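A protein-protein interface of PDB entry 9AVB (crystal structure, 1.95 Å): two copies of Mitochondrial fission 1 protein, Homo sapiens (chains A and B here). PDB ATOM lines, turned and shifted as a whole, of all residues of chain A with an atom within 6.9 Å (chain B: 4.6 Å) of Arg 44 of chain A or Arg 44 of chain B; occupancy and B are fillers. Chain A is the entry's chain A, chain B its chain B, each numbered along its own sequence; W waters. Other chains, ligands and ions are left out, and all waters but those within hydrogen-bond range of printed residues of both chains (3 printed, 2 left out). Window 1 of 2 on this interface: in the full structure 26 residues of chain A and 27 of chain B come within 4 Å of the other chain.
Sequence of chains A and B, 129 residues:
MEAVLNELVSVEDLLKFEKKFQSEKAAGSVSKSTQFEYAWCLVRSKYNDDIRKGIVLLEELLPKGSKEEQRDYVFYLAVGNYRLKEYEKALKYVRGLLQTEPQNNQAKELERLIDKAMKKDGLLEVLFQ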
ATOM      1  N   MET A   1      22.543 -11.210  38.471  1.00  0.00           N
ATOM      2  CA  MET A   1      21.952  -9.920  38.814  1.00  0.00           C
ATOM      3  C   MET A   1      20.692 -10.058  39.671  1.00  0.00           C
ATOM      4  O   MET A   1      19.941 -11.038  39.563  1.00  0.00           O
ATOM      5  CB  MET A   1      21.632  -9.128  37.539  1.00  0.00           C
ATOM      6  CG  MET A   1      22.885  -8.707  36.770  1.00  0.00           C
ATOM      7  SD  MET A   1      22.594  -7.789  35.246  1.00  0.00           S
ATOM      8  CE  MET A   1      20.892  -8.149  34.928  1.00  0.00           C
ATOM      9  N   LEU A   5      16.690  -5.767  38.293  1.00  0.00           N
ATOM     10  CA  LEU A   5      17.632  -5.466  37.220  1.00  0.00           C
ATOM     11  C   LEU A   5      17.546  -6.502  36.112  1.00  0.00           C
ATOM     12  O   LEU A   5      17.498  -6.160  34.924  1.00  0.00           O
ATOM     13  CB  LEU A   5      19.055  -5.415  37.766  1.00  0.00           C
ATOM     14  CG  LEU A   5      20.087  -4.914  36.764  1.00  0.00           C
ATOM     15  CD1 LEU A   5      19.688  -3.540  36.264  1.00  0.00           C
ATOM     16  CD2 LEU A   5      21.479  -4.893  37.376  1.00  0.00           C
ATOM     17  N   ASN A   6      17.562  -7.781  36.488  1.00  0.00           N
ATOM     18  CA  ASN A   6      17.518  -8.847  35.500  1.00  0.00           C
ATOM     19  C   ASN A   6      16.288  -8.720  34.615  1.00  0.00           C
ATOM     20  O   ASN A   6      16.356  -8.949  33.400  1.00  0.00           O
ATOM     21  CB  ASN A   6      17.547 -10.195  36.209  1.00  0.00           C
ATOM     22  CG  ASN A   6      17.640 -11.346  35.247  1.00  0.00           C
ATOM     23  OD1 ASN A   6      18.697 -11.598  34.667  1.00  0.00           O
ATOM     24  ND2 ASN A   6      16.539 -12.075  35.090  1.00  0.00           N
ATOM     25  N   VAL A   9      16.608  -5.636  32.095  1.00  0.00           N
ATOM     26  CA  VAL A   9      17.578  -5.930  31.046  1.00  0.00           C
ATOM     27  C   VAL A   9      17.016  -6.974  30.075  1.00  0.00           C
ATOM     28  O   VAL A   9      17.201  -6.879  28.852  1.00  0.00           O
ATOM     29  CB  VAL A   9      18.911  -6.361  31.692  1.00  0.00           C
ATOM     30  CG1 VAL A   9      19.868  -6.936  30.671  1.00  0.00           C
ATOM     31  CG2 VAL A   9      19.541  -5.153  32.420  1.00  0.00           C
ATOM     32  N   SER A  10      16.269  -7.950  30.590  1.00  0.00           N
ATOM     33  CA  SER A  10      15.669  -8.941  29.695  1.00  0.00           C
ATOM     34  C   SER A  10      14.703  -8.287  28.718  1.00  0.00           C
ATOM     35  O   SER A  10      14.669  -8.643  27.533  1.00  0.00           O
ATOM     36  CB  SER A  10      14.954 -10.014  30.503  1.00  0.00           C
ATOM     37  OG  SER A  10      15.911 -10.763  31.228  1.00  0.00           O
ATOM     38  N   ASP A  13      16.773  -6.315  26.009  1.00  0.00           N
ATOM     39  CA  ASP A  13      17.341  -7.250  25.036  1.00  0.00           C
ATOM     40  C   ASP A  13      16.306  -7.740  24.038  1.00  0.00           C
ATOM     41  O   ASP A  13      16.541  -7.706  22.826  1.00  0.00           O
ATOM     42  CB  ASP A  13      17.942  -8.462  25.762  1.00  0.00           C
ATOM     43  CG  ASP A  13      19.054  -8.088  26.694  1.00  0.00           C
ATOM     44  OD1 ASP A  13      19.691  -7.046  26.440  1.00  0.00           O
ATOM     45  OD2 ASP A  13      19.273  -8.811  27.691  1.00  0.00           O
ATOM     46  N   LEU A  14      15.197  -8.289  24.540  1.00  0.00           N
ATOM     47  CA  LEU A  14      14.161  -8.840  23.674  1.00  0.00           C
ATOM     48  C   LEU A  14      13.694  -7.810  22.648  1.00  0.00           C
ATOM     49  O   LEU A  14      13.673  -8.082  21.440  1.00  0.00           O
ATOM     50  CB  LEU A  14      13.005  -9.345  24.541  1.00  0.00           C
ATOM     51  CG  LEU A  14      11.761  -9.989  23.918  1.00  0.00           C
ATOM     52  CD1 LEU A  14      12.101 -11.171  23.016  1.00  0.00           C
ATOM     53  CD2 LEU A  14      10.829 -10.454  25.052  1.00  0.00           C
ATOM     54  N   TYR A  38      17.631 -13.417  18.868  1.00  0.00           N
ATOM     55  CA  TYR A  38      16.220 -13.219  19.155  1.00  0.00           C
ATOM     56  C   TYR A  38      15.634 -14.429  19.887  1.00  0.00           C
ATOM     57  O   TYR A  38      14.936 -14.279  20.904  1.00  0.00           O
ATOM     58  CB  TYR A  38      15.492 -12.916  17.841  1.00  0.00           C
ATOM     59  CG  TYR A  38      14.026 -12.595  17.950  1.00  0.00           C
ATOM     60  CD1 TYR A  38      13.526 -11.812  18.987  1.00  0.00           C
ATOM     61  CD2 TYR A  38      13.134 -13.053  16.984  1.00  0.00           C
ATOM     62  CE1 TYR A  38      12.163 -11.531  19.064  1.00  0.00           C
ATOM     63  CE2 TYR A  38      11.802 -12.769  17.049  1.00  0.00           C
ATOM     64  CZ  TYR A  38      11.317 -12.005  18.086  1.00  0.00           C
ATOM     65  OH  TYR A  38       9.980 -11.738  18.143  1.00  0.00           O
ATOM     66  N   ALA A  39      15.937 -15.641  19.405  1.00  0.00           N
ATOM     67  CA  ALA A  39      15.450 -16.858  20.064  1.00  0.00           C
ATOM     68  C   ALA A  39      15.958 -16.961  21.494  1.00  0.00           C
ATOM     69  O   ALA A  39      15.210 -17.331  22.412  1.00  0.00           O
ATOM     70  CB  ALA A  39      15.879 -18.101  19.277  1.00  0.00           C
ATOM     71  N   TRP A  40      17.240 -16.673  21.690  1.00  0.00           N
ATOM     72  CA  TRP A  40      17.815 -16.633  23.026  1.00  0.00           C
ATOM     73  C   TRP A  40      17.017 -15.717  23.953  1.00  0.00           C
ATOM     74  O   TRP A  40      16.724 -16.076  25.099  1.00  0.00           O
ATOM     75  CB  TRP A  40      19.281 -16.195  22.926  1.00  0.00           C
ATOM     76  CG  TRP A  40      19.933 -16.181  24.237  1.00  0.00           C
ATOM     77  CD1 TRP A  40      20.674 -17.170  24.805  1.00  0.00           C
ATOM     78  CD2 TRP A  40      19.889 -15.114  25.183  1.00  0.00           C
ATOM     79  NE1 TRP A  40      21.100 -16.778  26.057  1.00  0.00           N
ATOM     80  CE2 TRP A  40      20.628 -15.517  26.308  1.00  0.00           C
ATOM     81  CE3 TRP A  40      19.298 -13.845  25.185  1.00  0.00           C
ATOM     82  CZ2 TRP A  40      20.788 -14.700  27.419  1.00  0.00           C
ATOM     83  CZ3 TRP A  40      19.452 -13.042  26.296  1.00  0.00           C
ATOM     84  CH2 TRP A  40      20.187 -13.472  27.392  1.00  0.00           C
ATOM     85  N   CYS A  41      16.669 -14.518  23.477  1.00  0.00           N
ATOM     86  CA  CYS A  41      15.862 -13.608  24.289  1.00  0.00           C
ATOM     87  C   CYS A  41      14.464 -14.174  24.519  1.00  0.00           C
ATOM     88  O   CYS A  41      13.928 -14.104  25.634  1.00  0.00           O
ATOM     89  CB  CYS A  41      15.774 -12.238  23.602  1.00  0.00           C
ATOM     90  SG  CYS A  41      17.329 -11.335  23.503  1.00  0.00           S
ATOM     91  N   LEU A  42      13.858 -14.746  23.471  1.00  0.00           N
ATOM     92  CA  LEU A  42      12.487 -15.232  23.577  1.00  0.00           C
ATOM     93  C   LEU A  42      12.354 -16.355  24.597  1.00  0.00           C
ATOM     94  O   LEU A  42      11.378 -16.396  25.352  1.00  0.00           O
ATOM     95  CB  LEU A  42      11.991 -15.706  22.211  1.00  0.00           C
ATOM     96  CG  LEU A  42      11.645 -14.616  21.202  1.00  0.00           C
ATOM     97  CD1 LEU A  42      11.550 -15.232  19.825  1.00  0.00           C
ATOM     98  CD2 LEU A  42      10.303 -13.949  21.588  1.00  0.00           C
ATOM     99  N   VAL A  43      13.321 -17.278  24.631  1.00  0.00           N
ATOM    100  CA  VAL A  43      13.268 -18.393  25.569  1.00  0.00           C
ATOM    101  C   VAL A  43      13.370 -17.916  27.017  1.00  0.00           C
ATOM    102  O   VAL A  43      12.936 -18.619  27.938  1.00  0.00           O
ATOM    103  CB  VAL A  43      14.371 -19.420  25.192  1.00  0.00           C
ATOM    104  CG1 VAL A  43      15.042 -20.012  26.409  1.00  0.00           C
ATOM    105  CG2 VAL A  43      13.790 -20.522  24.317  1.00  0.00           C
ATOM    106  N   ARG A  44      13.874 -16.705  27.237  1.00  0.00           N
ATOM    107  CA  ARG A  44      14.012 -16.142  28.582  1.00  0.00           C
ATOM    108  C   ARG A  44      12.862 -15.218  28.978  1.00  0.00           C
ATOM    109  O   ARG A  44      12.848 -14.717  30.103  1.00  0.00           O
ATOM    110  CB  ARG A  44      15.338 -15.397  28.686  1.00  0.00           C
ATOM    111  CG  ARG A  44      16.511 -16.359  28.646  1.00  0.00           C
ATOM    112  CD  ARG A  44      17.779 -15.618  28.283  1.00  0.00           C
ATOM    113  NE  ARG A  44      18.570 -15.346  29.477  1.00  0.00           N
ATOM    114  CZ  ARG A  44      18.454 -14.257  30.229  1.00  0.00           C
ATOM    115  NH1 ARG A  44      17.665 -13.253  29.878  1.00  0.00           N
ATOM    116  NH2 ARG A  44      19.149 -14.173  31.361  1.00  0.00           N
ATOM    117  N   SER A  45      11.886 -15.025  28.101  1.00  0.00           N
ATOM    118  CA  SER A  45      10.805 -14.069  28.295  1.00  0.00           C
ATOM    119  C   SER A  45       9.851 -14.512  29.406  1.00  0.00           C
ATOM    120  O   SER A  45       9.721 -15.697  29.713  1.00  0.00           O
ATOM    121  CB  SER A  45      10.033 -13.915  26.979  1.00  0.00           C
ATOM    122  OG  SER A  45       8.794 -13.248  27.160  1.00  0.00           O
ATOM    123  N   LYS A  46       9.115 -13.546  29.970  1.00  0.00           N
ATOM    124  CA  LYS A  46       8.055 -13.935  30.900  1.00  0.00           C
ATOM    125  C   LYS A  46       6.794 -14.441  30.213  1.00  0.00           C
ATOM    126  O   LYS A  46       5.918 -14.970  30.905  1.00  0.00           O
ATOM    127  CB  LYS A  46       7.683 -12.781  31.826  1.00  0.00           C
ATOM    128  CG  LYS A  46       7.143 -11.565  31.114  1.00  0.00           C
ATOM    129  CD  LYS A  46       6.675 -10.542  32.130  1.00  0.00           C
ATOM    130  CE  LYS A  46       7.875  -9.772  32.611  1.00  0.00           C
ATOM    131  NZ  LYS A  46       8.388  -8.828  31.555  1.00  0.00           N
ATOM    132  N   TYR A  47       6.670 -14.342  28.890  1.00  0.00           N
ATOM    133  CA  TYR A  47       5.447 -14.766  28.215  1.00  0.00           C
ATOM    134  C   TYR A  47       5.635 -16.135  27.566  1.00  0.00           C
ATOM    135  O   TYR A  47       6.554 -16.315  26.764  1.00  0.00           O
ATOM    136  CB  TYR A  47       5.012 -13.759  27.141  1.00  0.00           C
ATOM    137  CG  TYR A  47       4.661 -12.370  27.654  1.00  0.00           C
ATOM    138  CD1 TYR A  47       5.643 -11.405  27.837  1.00  0.00           C
ATOM    139  CD2 TYR A  47       3.346 -12.045  28.006  1.00  0.00           C
ATOM    140  CE1 TYR A  47       5.324 -10.124  28.300  1.00  0.00           C
ATOM    141  CE2 TYR A  47       3.024 -10.781  28.489  1.00  0.00           C
ATOM    142  CZ  TYR A  47       4.015  -9.829  28.640  1.00  0.00           C
ATOM    143  OH  TYR A  47       3.693  -8.577  29.115  1.00  0.00           O
ATOM    144  N   ASP A  50       6.048 -16.174  23.840  1.00  0.00           N
ATOM    145  CA  ASP A  50       7.412 -15.838  23.453  1.00  0.00           C
ATOM    146  C   ASP A  50       8.302 -17.076  23.527  1.00  0.00           C
ATOM    147  O   ASP A  50       9.111 -17.323  22.632  1.00  0.00           O
ATOM    148  CB  ASP A  50       7.992 -14.766  24.376  1.00  0.00           C
ATOM    149  CG  ASP A  50       7.539 -13.352  24.048  1.00  0.00           C
ATOM    150  OD1 ASP A  50       6.849 -13.123  23.033  1.00  0.00           O
ATOM    151  OD2 ASP A  50       7.941 -12.453  24.814  1.00  0.00           O
ATOM    152  N   ILE A  51       8.222 -17.818  24.638  1.00  0.00           N
ATOM    153  CA  ILE A  51       9.073 -18.996  24.803  1.00  0.00           C
ATOM    154  C   ILE A  51       8.827 -19.969  23.666  1.00  0.00           C
ATOM    155  O   ILE A  51       9.764 -20.522  23.081  1.00  0.00           O
ATOM    156  CB  ILE A  51       8.836 -19.658  26.174  1.00  0.00           C
ATOM    157  CG1 ILE A  51       9.049 -18.661  27.312  1.00  0.00           C
ATOM    158  CG2 ILE A  51       9.790 -20.867  26.376  1.00  0.00           C
ATOM    159  CD1 ILE A  51       8.631 -19.241  28.660  1.00  0.00           C
ATOM    160  N   TYR A  76      19.700 -24.183  24.642  1.00  0.00           N
ATOM    161  CA  TYR A  76      18.572 -23.261  24.817  1.00  0.00           C
ATOM    162  C   TYR A  76      17.223 -23.915  24.519  1.00  0.00           C
ATOM    163  O   TYR A  76      16.199 -23.470  25.055  1.00  0.00           O
ATOM    164  CB  TYR A  76      18.805 -21.994  23.995  1.00  0.00           C
ATOM    165  CG  TYR A  76      19.966 -21.240  24.610  1.00  0.00           C
ATOM    166  CD1 TYR A  76      19.824 -20.579  25.825  1.00  0.00           C
ATOM    167  CD2 TYR A  76      21.229 -21.304  24.050  1.00  0.00           C
ATOM    168  CE1 TYR A  76      20.893 -19.946  26.426  1.00  0.00           C
ATOM    169  CE2 TYR A  76      22.307 -20.671  24.643  1.00  0.00           C
ATOM    170  CZ  TYR A  76      22.128 -19.998  25.827  1.00  0.00           C
ATOM    171  OH  TYR A  76      23.207 -19.366  26.407  1.00  0.00           O
ATOM    172  N   VAL A  79      16.464 -25.220  27.794  1.00  0.00           N
ATOM    173  CA  VAL A  79      15.999 -24.170  28.701  1.00  0.00           C
ATOM    174  C   VAL A  79      14.540 -23.835  28.416  1.00  0.00           C
ATOM    175  O   VAL A  79      13.708 -23.755  29.332  1.00  0.00           O
ATOM    176  CB  VAL A  79      16.887 -22.916  28.594  1.00  0.00           C
ATOM    177  CG1 VAL A  79      16.285 -21.772  29.418  1.00  0.00           C
ATOM    178  CG2 VAL A  79      18.320 -23.237  29.025  1.00  0.00           C
ATOM    179  N   GLY A  80      14.216 -23.627  27.139  1.00  0.00           N
ATOM    180  CA  GLY A  80      12.876 -23.197  26.797  1.00  0.00           C
ATOM    181  C   GLY A  80      11.845 -24.250  27.143  1.00  0.00           C
ATOM    182  O   GLY A  80      10.769 -23.935  27.660  1.00  0.00           O
ATOM    183  N   ARG A  83      11.203 -24.322  30.883  1.00  0.00           N
ATOM    184  CA  ARG A  83      10.371 -23.212  31.337  1.00  0.00           C
ATOM    185  C   ARG A  83       8.920 -23.365  30.901  1.00  0.00           C
ATOM    186  O   ARG A  83       8.036 -22.753  31.503  1.00  0.00           O
ATOM    187  CB  ARG A  83      10.937 -21.887  30.817  1.00  0.00           C
ATOM    188  CG  ARG A  83      12.285 -21.538  31.479  1.00  0.00           C
ATOM    189  CD  ARG A  83      12.758 -20.156  31.129  1.00  0.00           C
ATOM    190  NE  ARG A  83      12.019 -19.179  31.918  1.00  0.00           N
ATOM    191  CZ  ARG A  83      11.292 -18.196  31.408  1.00  0.00           C
ATOM    192  NH1 ARG A  83      11.278 -17.954  30.111  1.00  0.00           N
ATOM    193  NH2 ARG A  83      10.559 -17.439  32.222  1.00  0.00           N
ATOM    194  N   MET B   1      13.148 -15.112  34.841  1.00  0.00           N
ATOM    195  CA  MET B   1      13.648 -16.458  35.127  1.00  0.00           C
ATOM    196  C   MET B   1      13.997 -16.580  36.613  1.00  0.00           C
ATOM    197  O   MET B   1      14.514 -15.630  37.189  1.00  0.00           O
ATOM    198  CB  MET B   1      14.880 -16.761  34.273  1.00  0.00           C
ATOM    199  CG  MET B   1      14.658 -16.720  32.761  1.00  0.00           C
ATOM    200  SD  MET B   1      15.643 -17.992  31.935  1.00  0.00           S
ATOM    201  CE  MET B   1      17.272 -17.295  32.117  1.00  0.00           C
ATOM    202  N   ASN B   6      18.700 -18.452  35.954  1.00  0.00           N
ATOM    203  CA  ASN B   6      19.366 -17.260  35.447  1.00  0.00           C
ATOM    204  C   ASN B   6      20.881 -17.350  35.589  1.00  0.00           C
ATOM    205  O   ASN B   6      21.625 -16.940  34.691  1.00  0.00           O
ATOM    206  CB  ASN B   6      18.856 -16.020  36.173  1.00  0.00           C
ATOM    207  CG  ASN B   6      19.303 -14.753  35.502  1.00  0.00           C
ATOM    208  OD1 ASN B   6      18.811 -14.394  34.434  1.00  0.00           O
ATOM    209  ND2 ASN B   6      20.253 -14.063  36.121  1.00  0.00           N
ATOM    210  N   VAL B   9      22.357 -19.988  33.007  1.00  0.00           N
ATOM    211  CA  VAL B   9      22.320 -19.460  31.648  1.00  0.00           C
ATOM    212  C   VAL B   9      23.348 -18.335  31.466  1.00  0.00           C
ATOM    213  O   VAL B   9      23.991 -18.229  30.415  1.00  0.00           O
ATOM    214  CB  VAL B   9      20.884 -19.003  31.297  1.00  0.00           C
ATOM    215  CG1 VAL B   9      20.852 -18.366  29.924  1.00  0.00           C
ATOM    216  CG2 VAL B   9      19.911 -20.211  31.339  1.00  0.00           C
ATOM    217  N   SER B  10      23.517 -17.485  32.481  1.00  0.00           N
ATOM    218  CA  SER B  10      24.518 -16.422  32.403  1.00  0.00           C
ATOM    219  C   SER B  10      25.913 -16.995  32.172  1.00  0.00           C
ATOM    220  O   SER B  10      26.662 -16.517  31.310  1.00  0.00           O
ATOM    221  CB  SER B  10      24.482 -15.586  33.682  1.00  0.00           C
ATOM    222  OG  SER B  10      25.603 -14.727  33.766  1.00  0.00           O
ATOM    223  N   TRP B  40      28.167  -7.640  26.599  1.00  0.00           N
ATOM    224  CA  TRP B  40      26.852  -7.772  27.220  1.00  0.00           C
ATOM    225  C   TRP B  40      26.871  -8.877  28.283  1.00  0.00           C
ATOM    226  O   TRP B  40      26.352  -8.700  29.393  1.00  0.00           O
ATOM    227  CB  TRP B  40      25.803  -8.028  26.109  1.00  0.00           C
ATOM    228  CG  TRP B  40      24.421  -8.291  26.615  1.00  0.00           C
ATOM    229  CD1 TRP B  40      23.390  -7.393  26.714  1.00  0.00           C
ATOM    230  CD2 TRP B  40      23.940  -9.512  27.171  1.00  0.00           C
ATOM    231  NE1 TRP B  40      22.288  -7.998  27.269  1.00  0.00           N
ATOM    232  CE2 TRP B  40      22.602  -9.298  27.561  1.00  0.00           C
ATOM    233  CE3 TRP B  40      24.507 -10.776  27.365  1.00  0.00           C
ATOM    234  CZ2 TRP B  40      21.830 -10.303  28.135  1.00  0.00           C
ATOM    235  CZ3 TRP B  40      23.743 -11.764  27.934  1.00  0.00           C
ATOM    236  CH2 TRP B  40      22.426 -11.524  28.318  1.00  0.00           C
ATOM    237  N   CYS B  41      27.502 -10.022  27.972  1.00  0.00           N
ATOM    238  CA  CYS B  41      27.647 -11.081  28.981  1.00  0.00           C
ATOM    239  C   CYS B  41      28.526 -10.629  30.152  1.00  0.00           C
ATOM    240  O   CYS B  41      28.206 -10.893  31.323  1.00  0.00           O
ATOM    241  CB  CYS B  41      28.235 -12.337  28.339  1.00  0.00           C
ATOM    242  SG  CYS B  41      27.172 -13.148  27.160  1.00  0.00           S
ATOM    243  N   LEU B  42      29.639  -9.945  29.854  1.00  0.00           N
ATOM    244  CA  LEU B  42      30.536  -9.475  30.907  1.00  0.00           C
ATOM    245  C   LEU B  42      29.841  -8.547  31.903  1.00  0.00           C
ATOM    246  O   LEU B  42      30.079  -8.648  33.113  1.00  0.00           O
ATOM    247  CB  LEU B  42      31.735  -8.770  30.276  1.00  0.00           C
ATOM    248  CG  LEU B  42      32.689  -9.707  29.561  1.00  0.00           C
ATOM    249  CD1 LEU B  42      33.679  -8.863  28.751  1.00  0.00           C
ATOM    250  CD2 LEU B  42      33.426 -10.559  30.617  1.00  0.00           C
ATOM    251  N   VAL B  43      29.014  -7.607  31.430  1.00  0.00           N
ATOM    252  CA  VAL B  43      28.434  -6.655  32.382  1.00  0.00           C
ATOM    253  C   VAL B  43      27.367  -7.294  33.261  1.00  0.00           C
ATOM    254  O   VAL B  43      26.979  -6.703  34.276  1.00  0.00           O
ATOM    255  CB  VAL B  43      27.857  -5.384  31.701  1.00  0.00           C
ATOM    256  CG1 VAL B  43      28.943  -4.619  30.941  1.00  0.00           C
ATOM    257  CG2 VAL B  43      26.702  -5.700  30.779  1.00  0.00           C
ATOM    258  N   ARG B  44      26.905  -8.497  32.913  1.00  0.00           N
ATOM    259  CA  ARG B  44      25.980  -9.284  33.729  1.00  0.00           C
ATOM    260  C   ARG B  44      26.677 -10.285  34.645  1.00  0.00           C
ATOM    261  O   ARG B  44      25.995 -11.024  35.368  1.00  0.00           O
ATOM    262  CB  ARG B  44      25.017 -10.040  32.811  1.00  0.00           C
ATOM    263  CG  ARG B  44      24.413  -9.143  31.744  1.00  0.00           C
ATOM    264  CD  ARG B  44      22.939  -9.378  31.590  1.00  0.00           C
ATOM    265  NE  ARG B  44      22.675 -10.800  31.379  1.00  0.00           N
ATOM    266  CZ  ARG B  44      21.916 -11.561  32.161  1.00  0.00           C
ATOM    267  NH1 ARG B  44      21.288 -11.066  33.219  1.00  0.00           N
ATOM    268  NH2 ARG B  44      21.787 -12.854  31.877  1.00  0.00           N
ATOM    269  N   SER B  45      28.008 -10.335  34.624  1.00  0.00           N
ATOM    270  CA  SER B  45      28.745 -11.385  35.324  1.00  0.00           C
ATOM    271  C   SER B  45      28.705 -11.159  36.829  1.00  0.00           C
ATOM    272  O   SER B  45      28.510 -10.041  37.314  1.00  0.00           O
ATOM    273  CB  SER B  45      30.203 -11.437  34.837  1.00  0.00           C
ATOM    274  OG  SER B  45      31.045 -12.215  35.702  1.00  0.00           O
ATOM    275  N   LYS B  46      28.921 -12.239  37.581  1.00  0.00           N
ATOM    276  CA  LYS B  46      29.084 -12.090  39.027  1.00  0.00           C
ATOM    277  C   LYS B  46      30.459 -11.566  39.427  1.00  0.00           C
ATOM    278  O   LYS B  46      30.637 -11.195  40.587  1.00  0.00           O
ATOM    279  CB  LYS B  46      28.842 -13.419  39.750  1.00  0.00           C
ATOM    280  CG  LYS B  46      29.942 -14.422  39.544  1.00  0.00           C
ATOM    281  CD  LYS B  46      29.545 -15.806  40.052  1.00  0.00           C
ATOM    282  CE  LYS B  46      28.380 -16.348  39.245  1.00  0.00           C
ATOM    283  NZ  LYS B  46      28.499 -17.823  39.004  1.00  0.00           N
ATOM    284  N   ARG B  83      26.154  -1.653  38.505  1.00  0.00           N
ATOM    285  CA  ARG B  83      26.515  -2.854  39.252  1.00  0.00           C
ATOM    286  C   ARG B  83      27.852  -2.680  39.963  1.00  0.00           C
ATOM    287  O   ARG B  83      28.099  -3.325  40.984  1.00  0.00           O
ATOM    288  CB  ARG B  83      26.539  -4.054  38.311  1.00  0.00           C
ATOM    289  CG  ARG B  83      25.135  -4.423  37.831  1.00  0.00           C
ATOM    290  CD  ARG B  83      25.111  -5.720  37.075  1.00  0.00           C
ATOM    291  NE  ARG B  83      25.251  -6.821  38.012  1.00  0.00           N
ATOM    292  CZ  ARG B  83      26.110  -7.816  37.874  1.00  0.00           C
ATOM    293  NH1 ARG B  83      26.882  -7.910  36.811  1.00  0.00           N
ATOM    294  NH2 ARG B  83      26.188  -8.742  38.824  1.00  0.00           N
HETATM  295  O   HOH W   1      22.319 -14.495  37.786  1.00  0.00           O
HETATM  296  O   HOH W   2      25.238 -11.934  37.877  1.00  0.00           O
HETATM  297  O   HOH W   3      23.127 -12.223  35.553  1.00  0.00           O
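Hydrophobic or aromatic side chains of chain A that line the printed part of chain B: Met 1, Leu 5, Trp 40 and Tyr 76. Printed residues of chain B that touch a printed residue of chain A: Met 1, Asn 6, Val 9, Trp 40, Arg 44 and Arg 83. Hydrophobic or aromatic side chains of chain B that line the printed part of chain A: Met 1, Val 9 and Trp 40. Along chain B the printed residues that touch a printed residue of chain A span positions 1 to 83. Among the printed residues, no Asp or Glu carboxylate lies within 4 Å of a Lys or Arg side-chain nitrogen of the other chain.
Arg 44 of chain A touches just these residues of chain B: Met 1, Asn 6, Val 9 and Arg 44. Of chain A, only Met 1, Asn 6 and Arg 44 come within 4 Å of Arg 44 of chain B. Printed residues of chain B within 4 Å of Met 1 of chain A: Arg 44 and Arg 83. Of the printed residues of chain B, Tyr 76 of chain A touches Val 9 (3.8 Å). Of the printed residues of chain A, Trp 40 of chain B touches Asp 13 (2.9 Å) and Trp 40 (3.1 Å). Leu 42 of chain B touches none of the printed residues of chain A. The nearest printed residue of chain B that does not touch Arg 44 of chain A is Trp 40 of chain B (5.2 Å).
Among the printed residues, merely in contact across the chains: Trp 40 of chain A with Trp 40 of chain B (3.1 Å), Met 1 of chain A with Arg 83 of chain B (3.3 Å), Met 1 of chain A with Arg 44 of chain B (3.4 Å), Arg 44 of chain A with Met 1 of chain B (3.5 Å), Arg 83 of chain A with Met 1 of chain B (3.7 Å), Leu 5 of chain A with Arg 83 of chain B (3.7 Å), Arg 44 of chain A with Val 9 of chain B (3.8 Å) and Tyr 76 of chain A with Val 9 of chain B (3.8 Å).
Water W1 bridges the side-chain amide nitrogen of Asn 6 of chain B (2.7 Å) and the backbone NH of Met 1 of chain A (3.4 Å). Water W2 lies within hydrogen-bond range of O of Arg 44 of chain B, N of Met 1 of chain A and NH2 of Arg 83 of chain B. Water W3 lies within hydrogen-bond range of O of Arg 44 of chain B (3.1 Å), N of Met 1 of chain A (3.1 Å) and ND2 of Asn 6 of chain B (3.5 Å).
Met 1 of chain A touches Arg 44 of chain B, and with the chains exchanged Arg 44 of chain A touches Met 1 of chain B. Asn 6 of chain A touches Arg 44 of chain B, and with the chains exchanged Arg 44 of chain A touches Asn 6 of chain B. Trp 40 of chain B touches its own counterpart, Trp 40 of chain A. Arg 44 of chain B touches its own counterpart, Arg 44 of chain A. Positions printed for both chains: 1, 6, 9, 10, 40, 41, 42, 43, 44, 45, 46 and 83.
The side-chain amide oxygen of Asn 6 of chain A lies close to the side-chain amide oxygen of Asn 6 of chain B (2.8 Å). The side-chain amide oxygen of Asn 6 of chain A lies within hydrogen-bond range of the guanidinium group of Arg 44 of chain B (3.0 Å). The side-chain carboxylate of Asp 13 of chain A lies within hydrogen-bond range of the indole nitrogen of Trp 40 of chain B, at 2.9 Å. The guanidinium group (NH2) of Arg 44 of chain A sits at hydrogen-bond distance from the side-chain amide oxygen (OD1) of Asn 6 of chain B. The guanidinium group of Arg 44 of chain A lies close to the guanidinium group of Arg 44 of chain B (3.0 Å).
The side-chain hydroxyl of Ser 10 of chain A sits at hydrogen-bond distance from the backbone carbonyl oxygen of Asn 6 of chain A. The backbone carbonyl oxygen (O) of Asp 13 of chain A lies close to the side-chain sulfur (SG) of Cys 41 of chain A (3.8 Å). The backbone carbonyl oxygen (O) of Val 43 of chain B is in hydrogen-bond range of the guanidinium group (NH1) of Arg 83 of chain B, at 2.8 Å. O of Ser 45 of chain B is in hydrogen-bond range of NH1 of Arg 83 of chain B (2.7 Å).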
